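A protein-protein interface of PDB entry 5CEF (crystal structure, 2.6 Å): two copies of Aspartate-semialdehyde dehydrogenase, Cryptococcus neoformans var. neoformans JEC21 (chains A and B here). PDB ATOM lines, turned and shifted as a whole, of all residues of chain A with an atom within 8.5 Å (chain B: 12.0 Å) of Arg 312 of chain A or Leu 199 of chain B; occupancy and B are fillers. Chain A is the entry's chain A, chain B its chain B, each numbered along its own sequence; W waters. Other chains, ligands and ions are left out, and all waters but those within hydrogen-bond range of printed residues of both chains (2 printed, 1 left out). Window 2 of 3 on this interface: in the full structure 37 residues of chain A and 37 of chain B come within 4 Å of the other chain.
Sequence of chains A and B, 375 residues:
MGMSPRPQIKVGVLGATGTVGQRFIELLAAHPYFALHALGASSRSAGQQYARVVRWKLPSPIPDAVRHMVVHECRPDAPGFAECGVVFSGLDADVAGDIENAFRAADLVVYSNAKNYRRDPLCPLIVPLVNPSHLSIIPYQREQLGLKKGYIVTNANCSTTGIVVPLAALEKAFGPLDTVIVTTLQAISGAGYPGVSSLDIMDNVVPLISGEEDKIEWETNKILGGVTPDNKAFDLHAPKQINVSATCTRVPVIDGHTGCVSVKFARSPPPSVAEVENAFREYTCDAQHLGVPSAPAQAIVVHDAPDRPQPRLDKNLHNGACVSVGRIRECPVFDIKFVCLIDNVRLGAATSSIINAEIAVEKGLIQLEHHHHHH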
ATOM      1  N   VAL A 253      12.140 -17.906 -31.667  1.00  0.00           N
ATOM      2  CA  VAL A 253      13.179 -17.613 -30.700  1.00  0.00           C
ATOM      3  C   VAL A 253      13.184 -16.108 -30.492  1.00  0.00           C
ATOM      4  O   VAL A 253      13.037 -15.327 -31.441  1.00  0.00           O
ATOM      5  CB  VAL A 253      14.517 -18.057 -31.273  1.00  0.00           C
ATOM      6  CG1 VAL A 253      15.649 -17.671 -30.345  1.00  0.00           C
ATOM      7  CG2 VAL A 253      14.504 -19.561 -31.539  1.00  0.00           C
ATOM      8  N   ILE A 254      13.329 -15.678 -29.269  1.00  0.00           N
ATOM      9  CA  ILE A 254      13.247 -14.271 -28.958  1.00  0.00           C
ATOM     10  C   ILE A 254      14.465 -13.492 -29.418  1.00  0.00           C
ATOM     11  O   ILE A 254      14.314 -12.496 -30.155  1.00  0.00           O
ATOM     12  CB  ILE A 254      13.078 -14.073 -27.456  1.00  0.00           C
ATOM     13  CG1 ILE A 254      11.673 -14.425 -27.094  1.00  0.00           C
ATOM     14  CG2 ILE A 254      13.305 -12.639 -27.031  1.00  0.00           C
ATOM     15  CD1 ILE A 254      11.517 -14.773 -25.621  1.00  0.00           C
ATOM     16  N   ASP A 255      15.663 -13.956 -29.036  1.00  0.00           N
ATOM     17  CA  ASP A 255      16.901 -13.259 -29.376  1.00  0.00           C
ATOM     18  C   ASP A 255      17.925 -14.200 -29.940  1.00  0.00           C
ATOM     19  O   ASP A 255      18.022 -15.330 -29.489  1.00  0.00           O
ATOM     20  CB  ASP A 255      17.509 -12.665 -28.144  1.00  0.00           C
ATOM     21  CG  ASP A 255      16.667 -11.571 -27.539  1.00  0.00           C
ATOM     22  OD1 ASP A 255      16.146 -10.710 -28.295  1.00  0.00           O
ATOM     23  OD2 ASP A 255      16.611 -11.484 -26.292  1.00  0.00           O
ATOM     24  N   GLY A 256      18.718 -13.730 -30.900  1.00  0.00           N
ATOM     25  CA  GLY A 256      19.801 -14.540 -31.451  1.00  0.00           C
ATOM     26  C   GLY A 256      19.541 -15.008 -32.877  1.00  0.00           C
ATOM     27  O   GLY A 256      18.668 -15.822 -33.096  1.00  0.00           O
ATOM     28  N   HIS A 257      20.321 -14.499 -33.837  1.00  0.00           N
ATOM     29  CA  HIS A 257      20.208 -14.949 -35.223  1.00  0.00           C
ATOM     30  C   HIS A 257      21.276 -15.966 -35.484  1.00  0.00           C
ATOM     31  O   HIS A 257      22.450 -15.660 -35.376  1.00  0.00           O
ATOM     32  CB  HIS A 257      20.341 -13.785 -36.235  1.00  0.00           C
ATOM     33  CG  HIS A 257      19.286 -12.736 -36.099  1.00  0.00           C
ATOM     34  ND1 HIS A 257      18.047 -13.012 -35.588  1.00  0.00           N
ATOM     35  CD2 HIS A 257      19.268 -11.423 -36.421  1.00  0.00           C
ATOM     36  CE1 HIS A 257      17.308 -11.922 -35.588  1.00  0.00           C
ATOM     37  NE2 HIS A 257      18.025 -10.941 -36.087  1.00  0.00           N
ATOM     38  N   THR A 258      20.868 -17.136 -35.925  1.00  0.00           N
ATOM     39  CA  THR A 258      21.790 -18.220 -36.205  1.00  0.00           C
ATOM     40  C   THR A 258      21.978 -18.369 -37.705  1.00  0.00           C
ATOM     41  O   THR A 258      21.035 -18.187 -38.460  1.00  0.00           O
ATOM     42  CB  THR A 258      21.217 -19.507 -35.634  1.00  0.00           C
ATOM     43  OG1 THR A 258      21.011 -19.334 -34.218  1.00  0.00           O
ATOM     44  CG2 THR A 258      22.129 -20.653 -35.894  1.00  0.00           C
ATOM     45  N   ARG A 308      27.292 -26.160 -30.240  1.00  0.00           N
ATOM     46  CA  ARG A 308      27.255 -24.718 -29.936  1.00  0.00           C
ATOM     47  C   ARG A 308      27.791 -23.949 -31.142  1.00  0.00           C
ATOM     48  O   ARG A 308      28.594 -24.499 -31.900  1.00  0.00           O
ATOM     49  CB  ARG A 308      28.096 -24.422 -28.693  1.00  0.00           C
ATOM     50  CG  ARG A 308      27.670 -25.156 -27.436  1.00  0.00           C
ATOM     51  CD  ARG A 308      26.332 -24.664 -26.927  1.00  0.00           C
ATOM     52  NE  ARG A 308      26.468 -23.440 -26.139  1.00  0.00           N
ATOM     53  CZ  ARG A 308      26.759 -23.419 -24.840  1.00  0.00           C
ATOM     54  NH1 ARG A 308      26.938 -24.555 -24.177  1.00  0.00           N
ATOM     55  NH2 ARG A 308      26.888 -22.258 -24.191  1.00  0.00           N
ATOM     56  N   PRO A 309      27.374 -22.687 -31.317  1.00  0.00           N
ATOM     57  CA  PRO A 309      26.564 -21.867 -30.436  1.00  0.00           C
ATOM     58  C   PRO A 309      25.102 -22.182 -30.483  1.00  0.00           C
ATOM     59  O   PRO A 309      24.650 -22.745 -31.462  1.00  0.00           O
ATOM     60  CB  PRO A 309      26.797 -20.468 -30.970  1.00  0.00           C
ATOM     61  CG  PRO A 309      27.050 -20.679 -32.398  1.00  0.00           C
ATOM     62  CD  PRO A 309      27.910 -21.899 -32.419  1.00  0.00           C
ATOM     63  N   GLN A 310      24.397 -21.781 -29.424  1.00  0.00           N
ATOM     64  CA  GLN A 310      22.948 -21.834 -29.357  1.00  0.00           C
ATOM     65  C   GLN A 310      22.472 -20.478 -28.908  1.00  0.00           C
ATOM     66  O   GLN A 310      22.999 -19.940 -27.940  1.00  0.00           O
ATOM     67  CB  GLN A 310      22.493 -22.853 -28.328  1.00  0.00           C
ATOM     68  CG  GLN A 310      22.749 -24.274 -28.735  1.00  0.00           C
ATOM     69  CD  GLN A 310      22.405 -25.260 -27.646  1.00  0.00           C
ATOM     70  OE1 GLN A 310      21.536 -25.017 -26.819  1.00  0.00           O
ATOM     71  NE2 GLN A 310      23.088 -26.364 -27.638  1.00  0.00           N
ATOM     72  N   PRO A 311      21.471 -19.895 -29.587  1.00  0.00           N
ATOM     73  CA  PRO A 311      21.074 -18.486 -29.307  1.00  0.00           C
ATOM     74  C   PRO A 311      20.646 -18.228 -27.868  1.00  0.00           C
ATOM     75  O   PRO A 311      20.951 -17.187 -27.322  1.00  0.00           O
ATOM     76  CB  PRO A 311      19.916 -18.253 -30.260  1.00  0.00           C
ATOM     77  CG  PRO A 311      19.479 -19.607 -30.690  1.00  0.00           C
ATOM     78  CD  PRO A 311      20.716 -20.445 -30.709  1.00  0.00           C
ATOM     79  N   ARG A 312      19.982 -19.181 -27.243  1.00  0.00           N
ATOM     80  CA  ARG A 312      19.524 -18.997 -25.859  1.00  0.00           C
ATOM     81  C   ARG A 312      20.642 -19.157 -24.857  1.00  0.00           C
ATOM     82  O   ARG A 312      20.619 -18.526 -23.835  1.00  0.00           O
ATOM     83  CB  ARG A 312      18.403 -19.976 -25.483  1.00  0.00           C
ATOM     84  CG  ARG A 312      17.748 -19.570 -24.181  1.00  0.00           C
ATOM     85  CD  ARG A 312      16.493 -20.355 -23.800  1.00  0.00           C
ATOM     86  NE  ARG A 312      16.714 -21.759 -23.458  1.00  0.00           N
ATOM     87  CZ  ARG A 312      17.334 -22.180 -22.370  1.00  0.00           C
ATOM     88  NH1 ARG A 312      17.811 -21.298 -21.478  1.00  0.00           N
ATOM     89  NH2 ARG A 312      17.477 -23.483 -22.152  1.00  0.00           N
ATOM     90  N   LEU A 313      21.622 -19.982 -25.152  1.00  0.00           N
ATOM     91  CA  LEU A 313      22.729 -20.179 -24.233  1.00  0.00           C
ATOM     92  C   LEU A 313      23.859 -19.150 -24.385  1.00  0.00           C
ATOM     93  O   LEU A 313      24.458 -18.743 -23.395  1.00  0.00           O
ATOM     94  CB  LEU A 313      23.316 -21.558 -24.417  1.00  0.00           C
ATOM     95  CG  LEU A 313      22.762 -22.776 -23.693  1.00  0.00           C
ATOM     96  CD1 LEU A 313      21.277 -22.684 -23.520  1.00  0.00           C
ATOM     97  CD2 LEU A 313      23.206 -24.089 -24.322  1.00  0.00           C
ATOM     98  N   ASP A 314      24.102 -18.674 -25.606  1.00  0.00           N
ATOM     99  CA  ASP A 314      25.287 -17.894 -25.902  1.00  0.00           C
ATOM    100  C   ASP A 314      25.000 -16.431 -26.170  1.00  0.00           C
ATOM    101  O   ASP A 314      25.648 -15.774 -26.969  1.00  0.00           O
ATOM    102  CB  ASP A 314      26.055 -18.569 -27.045  1.00  0.00           C
ATOM    103  CG  ASP A 314      26.510 -19.975 -26.681  1.00  0.00           C
ATOM    104  OD1 ASP A 314      27.224 -20.074 -25.666  1.00  0.00           O
ATOM    105  OD2 ASP A 314      26.163 -20.966 -27.368  1.00  0.00           O
ATOM    106  N   LYS A 315      24.055 -15.885 -25.450  1.00  0.00           N
ATOM    107  CA  LYS A 315      23.882 -14.436 -25.443  1.00  0.00           C
ATOM    108  C   LYS A 315      24.615 -13.894 -24.216  1.00  0.00           C
ATOM    109  O   LYS A 315      24.896 -14.628 -23.269  1.00  0.00           O
ATOM    110  CB  LYS A 315      22.403 -14.053 -25.442  1.00  0.00           C
ATOM    111  CG  LYS A 315      21.602 -14.505 -24.226  1.00  0.00           C
ATOM    112  CD  LYS A 315      20.138 -14.580 -24.601  1.00  0.00           C
ATOM    113  CE  LYS A 315      19.236 -14.922 -23.431  1.00  0.00           C
ATOM    114  NZ  LYS A 315      17.842 -14.904 -23.947  1.00  0.00           N
ATOM    115  N   ASN A 316      24.923 -12.600 -24.282  1.00  0.00           N
ATOM    116  CA  ASN A 316      25.684 -11.874 -23.264  1.00  0.00           C
ATOM    117  C   ASN A 316      26.992 -12.545 -22.927  1.00  0.00           C
ATOM    118  O   ASN A 316      27.286 -12.796 -21.777  1.00  0.00           O
ATOM    119  CB  ASN A 316      24.847 -11.634 -22.015  1.00  0.00           C
ATOM    120  CG  ASN A 316      23.541 -10.935 -22.329  1.00  0.00           C
ATOM    121  OD1 ASN A 316      23.473 -10.035 -23.179  1.00  0.00           O
ATOM    122  ND2 ASN A 316      22.486 -11.371 -21.666  1.00  0.00           N
ATOM    123  N   LEU A 341      26.459 -17.118 -34.824  1.00  0.00           N
ATOM    124  CA  LEU A 341      25.424 -16.529 -34.034  1.00  0.00           C
ATOM    125  C   LEU A 341      25.740 -15.083 -33.811  1.00  0.00           C
ATOM    126  O   LEU A 341      26.855 -14.745 -33.438  1.00  0.00           O
ATOM    127  CB  LEU A 341      25.360 -17.209 -32.673  1.00  0.00           C
ATOM    128  CG  LEU A 341      24.429 -16.548 -31.649  1.00  0.00           C
ATOM    129  CD1 LEU A 341      22.972 -16.650 -32.076  1.00  0.00           C
ATOM    130  CD2 LEU A 341      24.636 -17.225 -30.297  1.00  0.00           C
ATOM    131  N   ILE B 188      10.633 -31.534 -33.349  1.00  0.00           N
ATOM    132  CA  ILE B 188      11.006 -32.411 -32.227  1.00  0.00           C
ATOM    133  C   ILE B 188      10.362 -33.797 -32.280  1.00  0.00           C
ATOM    134  O   ILE B 188      10.891 -34.707 -31.677  1.00  0.00           O
ATOM    135  CB  ILE B 188      10.793 -31.746 -30.836  1.00  0.00           C
ATOM    136  CG1 ILE B 188       9.334 -31.522 -30.530  1.00  0.00           C
ATOM    137  CG2 ILE B 188      11.434 -30.376 -30.754  1.00  0.00           C
ATOM    138  CD1 ILE B 188       8.734 -32.575 -29.628  1.00  0.00           C
ATOM    139  N   GLY B 195      14.328 -38.577 -25.861  1.00  0.00           N
ATOM    140  CA  GLY B 195      14.127 -37.651 -27.010  1.00  0.00           C
ATOM    141  C   GLY B 195      14.686 -36.263 -26.723  1.00  0.00           C
ATOM    142  O   GLY B 195      15.742 -36.178 -26.075  1.00  0.00           O
ATOM    143  N   VAL B 196      14.006 -35.194 -27.176  1.00  0.00           N
ATOM    144  CA  VAL B 196      14.415 -33.785 -26.885  1.00  0.00           C
ATOM    145  C   VAL B 196      13.720 -33.165 -25.661  1.00  0.00           C
ATOM    146  O   VAL B 196      12.501 -33.072 -25.580  1.00  0.00           O
ATOM    147  CB  VAL B 196      14.069 -32.836 -28.034  1.00  0.00           C
ATOM    148  CG1 VAL B 196      14.492 -31.402 -27.731  1.00  0.00           C
ATOM    149  CG2 VAL B 196      14.687 -33.324 -29.316  1.00  0.00           C
ATOM    150  N   SER B 197      14.509 -32.742 -24.697  1.00  0.00           N
ATOM    151  CA  SER B 197      13.961 -32.216 -23.473  1.00  0.00           C
ATOM    152  C   SER B 197      13.587 -30.774 -23.694  1.00  0.00           C
ATOM    153  O   SER B 197      14.218 -30.061 -24.484  1.00  0.00           O
ATOM    154  CB  SER B 197      14.969 -32.337 -22.346  1.00  0.00           C
ATOM    155  OG  SER B 197      15.936 -31.313 -22.467  1.00  0.00           O
ATOM    156  N   SER B 198      12.568 -30.322 -22.984  1.00  0.00           N
ATOM    157  CA  SER B 198      12.088 -28.980 -23.208  1.00  0.00           C
ATOM    158  C   SER B 198      13.162 -27.963 -22.849  1.00  0.00           C
ATOM    159  O   SER B 198      13.325 -26.949 -23.518  1.00  0.00           O
ATOM    160  CB  SER B 198      10.781 -28.740 -22.459  1.00  0.00           C
ATOM    161  OG  SER B 198      10.995 -28.813 -21.074  1.00  0.00           O
ATOM    162  N   LEU B 199      13.948 -28.271 -21.849  1.00  0.00           N
ATOM    163  CA  LEU B 199      15.069 -27.423 -21.504  1.00  0.00           C
ATOM    164  C   LEU B 199      16.081 -27.227 -22.609  1.00  0.00           C
ATOM    165  O   LEU B 199      16.675 -26.169 -22.675  1.00  0.00           O
ATOM    166  CB  LEU B 199      15.822 -27.996 -20.319  1.00  0.00           C
ATOM    167  CG  LEU B 199      15.654 -27.268 -19.002  1.00  0.00           C
ATOM    168  CD1 LEU B 199      16.467 -28.019 -17.941  1.00  0.00           C
ATOM    169  CD2 LEU B 199      16.105 -25.813 -19.114  1.00  0.00           C
ATOM    170  N   ASP B 200      16.309 -28.239 -23.449  1.00  0.00           N
ATOM    171  CA  ASP B 200      17.303 -28.142 -24.503  1.00  0.00           C
ATOM    172  C   ASP B 200      16.846 -27.228 -25.593  1.00  0.00           C
ATOM    173  O   ASP B 200      17.677 -26.575 -26.204  1.00  0.00           O
ATOM    174  CB  ASP B 200      17.617 -29.501 -25.127  1.00  0.00           C
ATOM    175  CG  ASP B 200      18.381 -30.446 -24.176  1.00  0.00           C
ATOM    176  OD1 ASP B 200      19.069 -29.951 -23.250  1.00  0.00           O
ATOM    177  OD2 ASP B 200      18.254 -31.700 -24.359  1.00  0.00           O
ATOM    178  N   ILE B 201      15.531 -27.182 -25.839  1.00  0.00           N
ATOM    179  CA  ILE B 201      15.005 -26.623 -27.082  1.00  0.00           C
ATOM    180  C   ILE B 201      14.103 -25.381 -26.977  1.00  0.00           C
ATOM    181  O   ILE B 201      14.050 -24.616 -27.950  1.00  0.00           O
ATOM    182  CB  ILE B 201      14.294 -27.722 -27.921  1.00  0.00           C
ATOM    183  CG1 ILE B 201      14.029 -27.281 -29.358  1.00  0.00           C
ATOM    184  CG2 ILE B 201      12.991 -28.148 -27.286  1.00  0.00           C
ATOM    185  CD1 ILE B 201      15.294 -26.958 -30.124  1.00  0.00           C
ATOM    186  N   MET B 202      13.437 -25.130 -25.854  1.00  0.00           N
ATOM    187  CA  MET B 202      12.493 -24.009 -25.811  1.00  0.00           C
ATOM    188  C   MET B 202      13.177 -22.689 -26.045  1.00  0.00           C
ATOM    189  O   MET B 202      14.264 -22.471 -25.535  1.00  0.00           O
ATOM    190  CB  MET B 202      11.746 -23.931 -24.479  1.00  0.00           C
ATOM    191  CG  MET B 202      10.789 -25.088 -24.233  1.00  0.00           C
ATOM    192  SD  MET B 202       9.724 -24.963 -22.778  1.00  0.00           S
ATOM    193  CE  MET B 202      10.676 -23.935 -21.708  1.00  0.00           C
ATOM    194  N   ASP B 203      12.597 -21.826 -26.880  1.00  0.00           N
ATOM    195  CA  ASP B 203      13.202 -20.504 -27.134  1.00  0.00           C
ATOM    196  C   ASP B 203      14.682 -20.609 -27.606  1.00  0.00           C
ATOM    197  O   ASP B 203      15.530 -19.778 -27.266  1.00  0.00           O
ATOM    198  CB  ASP B 203      13.121 -19.623 -25.876  1.00  0.00           C
ATOM    199  CG  ASP B 203      13.550 -18.158 -26.145  1.00  0.00           C
ATOM    200  OD1 ASP B 203      13.383 -17.684 -27.264  1.00  0.00           O
ATOM    201  OD2 ASP B 203      14.052 -17.477 -25.232  1.00  0.00           O
ATOM    202  N   ASN B 204      14.964 -21.620 -28.412  1.00  0.00           N
ATOM    203  CA  ASN B 204      16.326 -21.938 -28.763  1.00  0.00           C
ATOM    204  C   ASN B 204      16.467 -22.682 -30.128  1.00  0.00           C
ATOM    205  O   ASN B 204      15.482 -23.054 -30.765  1.00  0.00           O
ATOM    206  CB  ASN B 204      16.907 -22.762 -27.619  1.00  0.00           C
ATOM    207  CG  ASN B 204      18.433 -22.887 -27.677  1.00  0.00           C
ATOM    208  OD1 ASN B 204      19.143 -21.977 -28.100  1.00  0.00           O
ATOM    209  ND2 ASN B 204      18.924 -24.049 -27.287  1.00  0.00           N
ATOM    210  N   VAL B 205      17.701 -22.854 -30.572  1.00  0.00           N
ATOM    211  CA  VAL B 205      18.025 -23.686 -31.728  1.00  0.00           C
ATOM    212  C   VAL B 205      19.221 -24.524 -31.335  1.00  0.00           C
ATOM    213  O   VAL B 205      20.131 -24.009 -30.707  1.00  0.00           O
ATOM    214  CB  VAL B 205      18.416 -22.805 -32.946  1.00  0.00           C
ATOM    215  CG1 VAL B 205      19.081 -23.629 -34.026  1.00  0.00           C
ATOM    216  CG2 VAL B 205      17.203 -22.050 -33.489  1.00  0.00           C
ATOM    217  N   VAL B 206      19.182 -25.810 -31.638  1.00  0.00           N
ATOM    218  CA  VAL B 206      20.281 -26.712 -31.353  1.00  0.00           C
ATOM    219  C   VAL B 206      20.846 -27.090 -32.695  1.00  0.00           C
ATOM    220  O   VAL B 206      20.198 -27.772 -33.464  1.00  0.00           O
ATOM    221  CB  VAL B 206      19.844 -27.988 -30.586  1.00  0.00           C
ATOM    222  CG1 VAL B 206      21.040 -28.883 -30.337  1.00  0.00           C
ATOM    223  CG2 VAL B 206      19.295 -27.604 -29.233  1.00  0.00           C
ATOM    224  N   PRO B 207      22.054 -26.621 -32.997  1.00  0.00           N
ATOM    225  CA  PRO B 207      22.575 -26.802 -34.343  1.00  0.00           C
ATOM    226  C   PRO B 207      23.266 -28.130 -34.589  1.00  0.00           C
ATOM    227  O   PRO B 207      24.087 -28.211 -35.502  1.00  0.00           O
ATOM    228  CB  PRO B 207      23.598 -25.659 -34.450  1.00  0.00           C
ATOM    229  CG  PRO B 207      24.144 -25.565 -33.071  1.00  0.00           C
ATOM    230  CD  PRO B 207      22.962 -25.817 -32.159  1.00  0.00           C
ATOM    231  N   ARG B 250      17.862 -28.391 -35.035  1.00  0.00           N
ATOM    232  CA  ARG B 250      16.617 -28.649 -34.367  1.00  0.00           C
ATOM    233  C   ARG B 250      16.005 -27.329 -33.956  1.00  0.00           C
ATOM    234  O   ARG B 250      16.697 -26.461 -33.474  1.00  0.00           O
ATOM    235  CB  ARG B 250      16.847 -29.482 -33.132  1.00  0.00           C
ATOM    236  CG  ARG B 250      15.588 -29.889 -32.393  1.00  0.00           C
ATOM    237  CD  ARG B 250      14.997 -31.145 -33.012  1.00  0.00           C
ATOM    238  NE  ARG B 250      15.817 -32.331 -32.759  1.00  0.00           N
ATOM    239  CZ  ARG B 250      15.692 -33.497 -33.406  1.00  0.00           C
ATOM    240  NH1 ARG B 250      14.814 -33.651 -34.379  1.00  0.00           N
ATOM    241  NH2 ARG B 250      16.502 -34.501 -33.113  1.00  0.00           N
ATOM    242  N   VAL B 251      14.686 -27.212 -34.118  1.00  0.00           N
ATOM    243  CA  VAL B 251      13.975 -25.995 -33.804  1.00  0.00           C
ATOM    244  C   VAL B 251      12.805 -26.341 -32.919  1.00  0.00           C
ATOM    245  O   VAL B 251      12.424 -27.478 -32.849  1.00  0.00           O
ATOM    246  CB  VAL B 251      13.473 -25.285 -35.088  1.00  0.00           C
ATOM    247  CG1 VAL B 251      14.634 -24.723 -35.904  1.00  0.00           C
ATOM    248  CG2 VAL B 251      12.673 -26.226 -35.964  1.00  0.00           C
ATOM    249  N   PRO B 252      12.209 -25.344 -32.231  1.00  0.00           N
ATOM    250  CA  PRO B 252      11.123 -25.623 -31.282  1.00  0.00           C
ATOM    251  C   PRO B 252       9.758 -25.709 -31.945  1.00  0.00           C
ATOM    252  O   PRO B 252       8.914 -24.809 -31.777  1.00  0.00           O
ATOM    253  CB  PRO B 252      11.189 -24.452 -30.313  1.00  0.00           C
ATOM    254  CG  PRO B 252      12.006 -23.405 -30.942  1.00  0.00           C
ATOM    255  CD  PRO B 252      12.616 -23.932 -32.198  1.00  0.00           C
ATOM    256  N   VAL B 253       9.581 -26.788 -32.697  1.00  0.00           N
ATOM    257  CA  VAL B 253       8.417 -27.012 -33.496  1.00  0.00           C
ATOM    258  C   VAL B 253       8.060 -28.473 -33.322  1.00  0.00           C
ATOM    259  O   VAL B 253       8.945 -29.342 -33.271  1.00  0.00           O
ATOM    260  CB  VAL B 253       8.710 -26.753 -34.981  1.00  0.00           C
ATOM    261  CG1 VAL B 253       7.509 -27.118 -35.807  1.00  0.00           C
ATOM    262  CG2 VAL B 253       9.096 -25.308 -35.196  1.00  0.00           C
HETATM  263  O   HOH W   1      20.369 -27.254 -25.235  1.00  0.00           O
HETATM  264  O   HOH W   2      16.900 -16.699 -27.215  1.00  0.00           O
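OD1 of Asn 204 of chain B sits close to N of Pro 311 of chain A, at 3.5 Å.
The guanidinium group (NE) of Arg 312 of chain A sits at hydrogen-bond distance from the backbone carbonyl oxygen (O) of Met 202 of chain B, 3.3 Å away.
OD1 of Asn 204 of chain B is in hydrogen-bond range of N of Arg 312 of chain A (3.0 Å).
The side-chain amide oxygen (OE1) of Gln 310 of chain A lies within hydrogen-bond range of the side-chain amide nitrogen (ND2) of Asn 204 of chain B (2.8 Å).
The guanidinium group of Arg 312 of chain A lies within hydrogen-bond range of the backbone carbonyl oxygen of Leu 199 of chain B.
OD1 of Asp 203 of chain B lies within hydrogen-bond range of N of Ile 254 of chain A, at 2.8 Å.
N of Gln 310 of chain A lies within hydrogen-bond range of OD2 of Asp 314 of chain A.
ND2 of Asn 204 of chain B lies within hydrogen-bond range of O of Asp 200 of chain B (3.0 Å).
OD1 of Asp 203 of chain B touches CA of Val 253 of chain A, 3.4 Å away.
CG2 of Val 253 of chain A touches O of Asn 204 of chain B, at 3.7 Å.
Pro 207 of chain B touches Pro 309 of chain A (CG to O, 3.3 Å).
O of Val 205 of chain B touches CG of Gln 310 of chain A (3.3 Å).
Gln 310 of chain A touches Pro 207 of chain B.
Val 205 of chain B touches Pro 311 of chain A.
Asp 203 of chain B touches Arg 312 of chain A (O to CB, 3.4 Å).
Of the printed residues of chain B, Val 253 of chain A touches Asp 203 and Asn 204.
Of the printed residues of chain B, Ile 254 of chain A touches Asp 203.
No residue of chain B comes within 4 Å of Gly 256 of chain A.
Of the printed residues of chain B, Pro 309 of chain A touches Pro 207.
Gln 310 of chain A touches just these residues of chain B: Asn 204, Val 205 and Pro 207.
Arg 312 of chain A touches just these residues of chain B: Leu 199, Met 202, Asp 203 and Asn 204.
No residue of chain B comes within 4 Å of Leu 313 of chain A.
No residue of chain B comes within 4 Å of Asp 314 of chain A.
No residue of chain B comes within 4 Å of Lys 315 of chain A.
Leu 199 of chain B touches just one residue of chain A: Arg 312 (2.9 Å).
Asp 200 of chain B touches none of the printed residues of chain A.
Arg 250 of chain B touches none of the printed residues of chain A.
The nearest printed residue of chain A that does not touch Pro 207 of chain B is Arg 308 of chain A (4.3 Å).
Hydrophobic or aromatic side chains of chain B that line the printed part of chain A: Val 205 and Pro 207.
Among the printed residues, 13 pairs touch across the chains.
1 position is printed for both chains.
Water W2 lies within hydrogen-bond range of O of Asp 255 of chain A (2.9 Å) and O of Asp 203 of chain B (3.4 Å).
Water W1 lies within hydrogen-bond range of the backbone carbonyl oxygen (O) of Asp 200 of chain B (2.9 Å) and the side-chain amide oxygen (OE1) of Gln 310 of chain A (3.0 Å).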
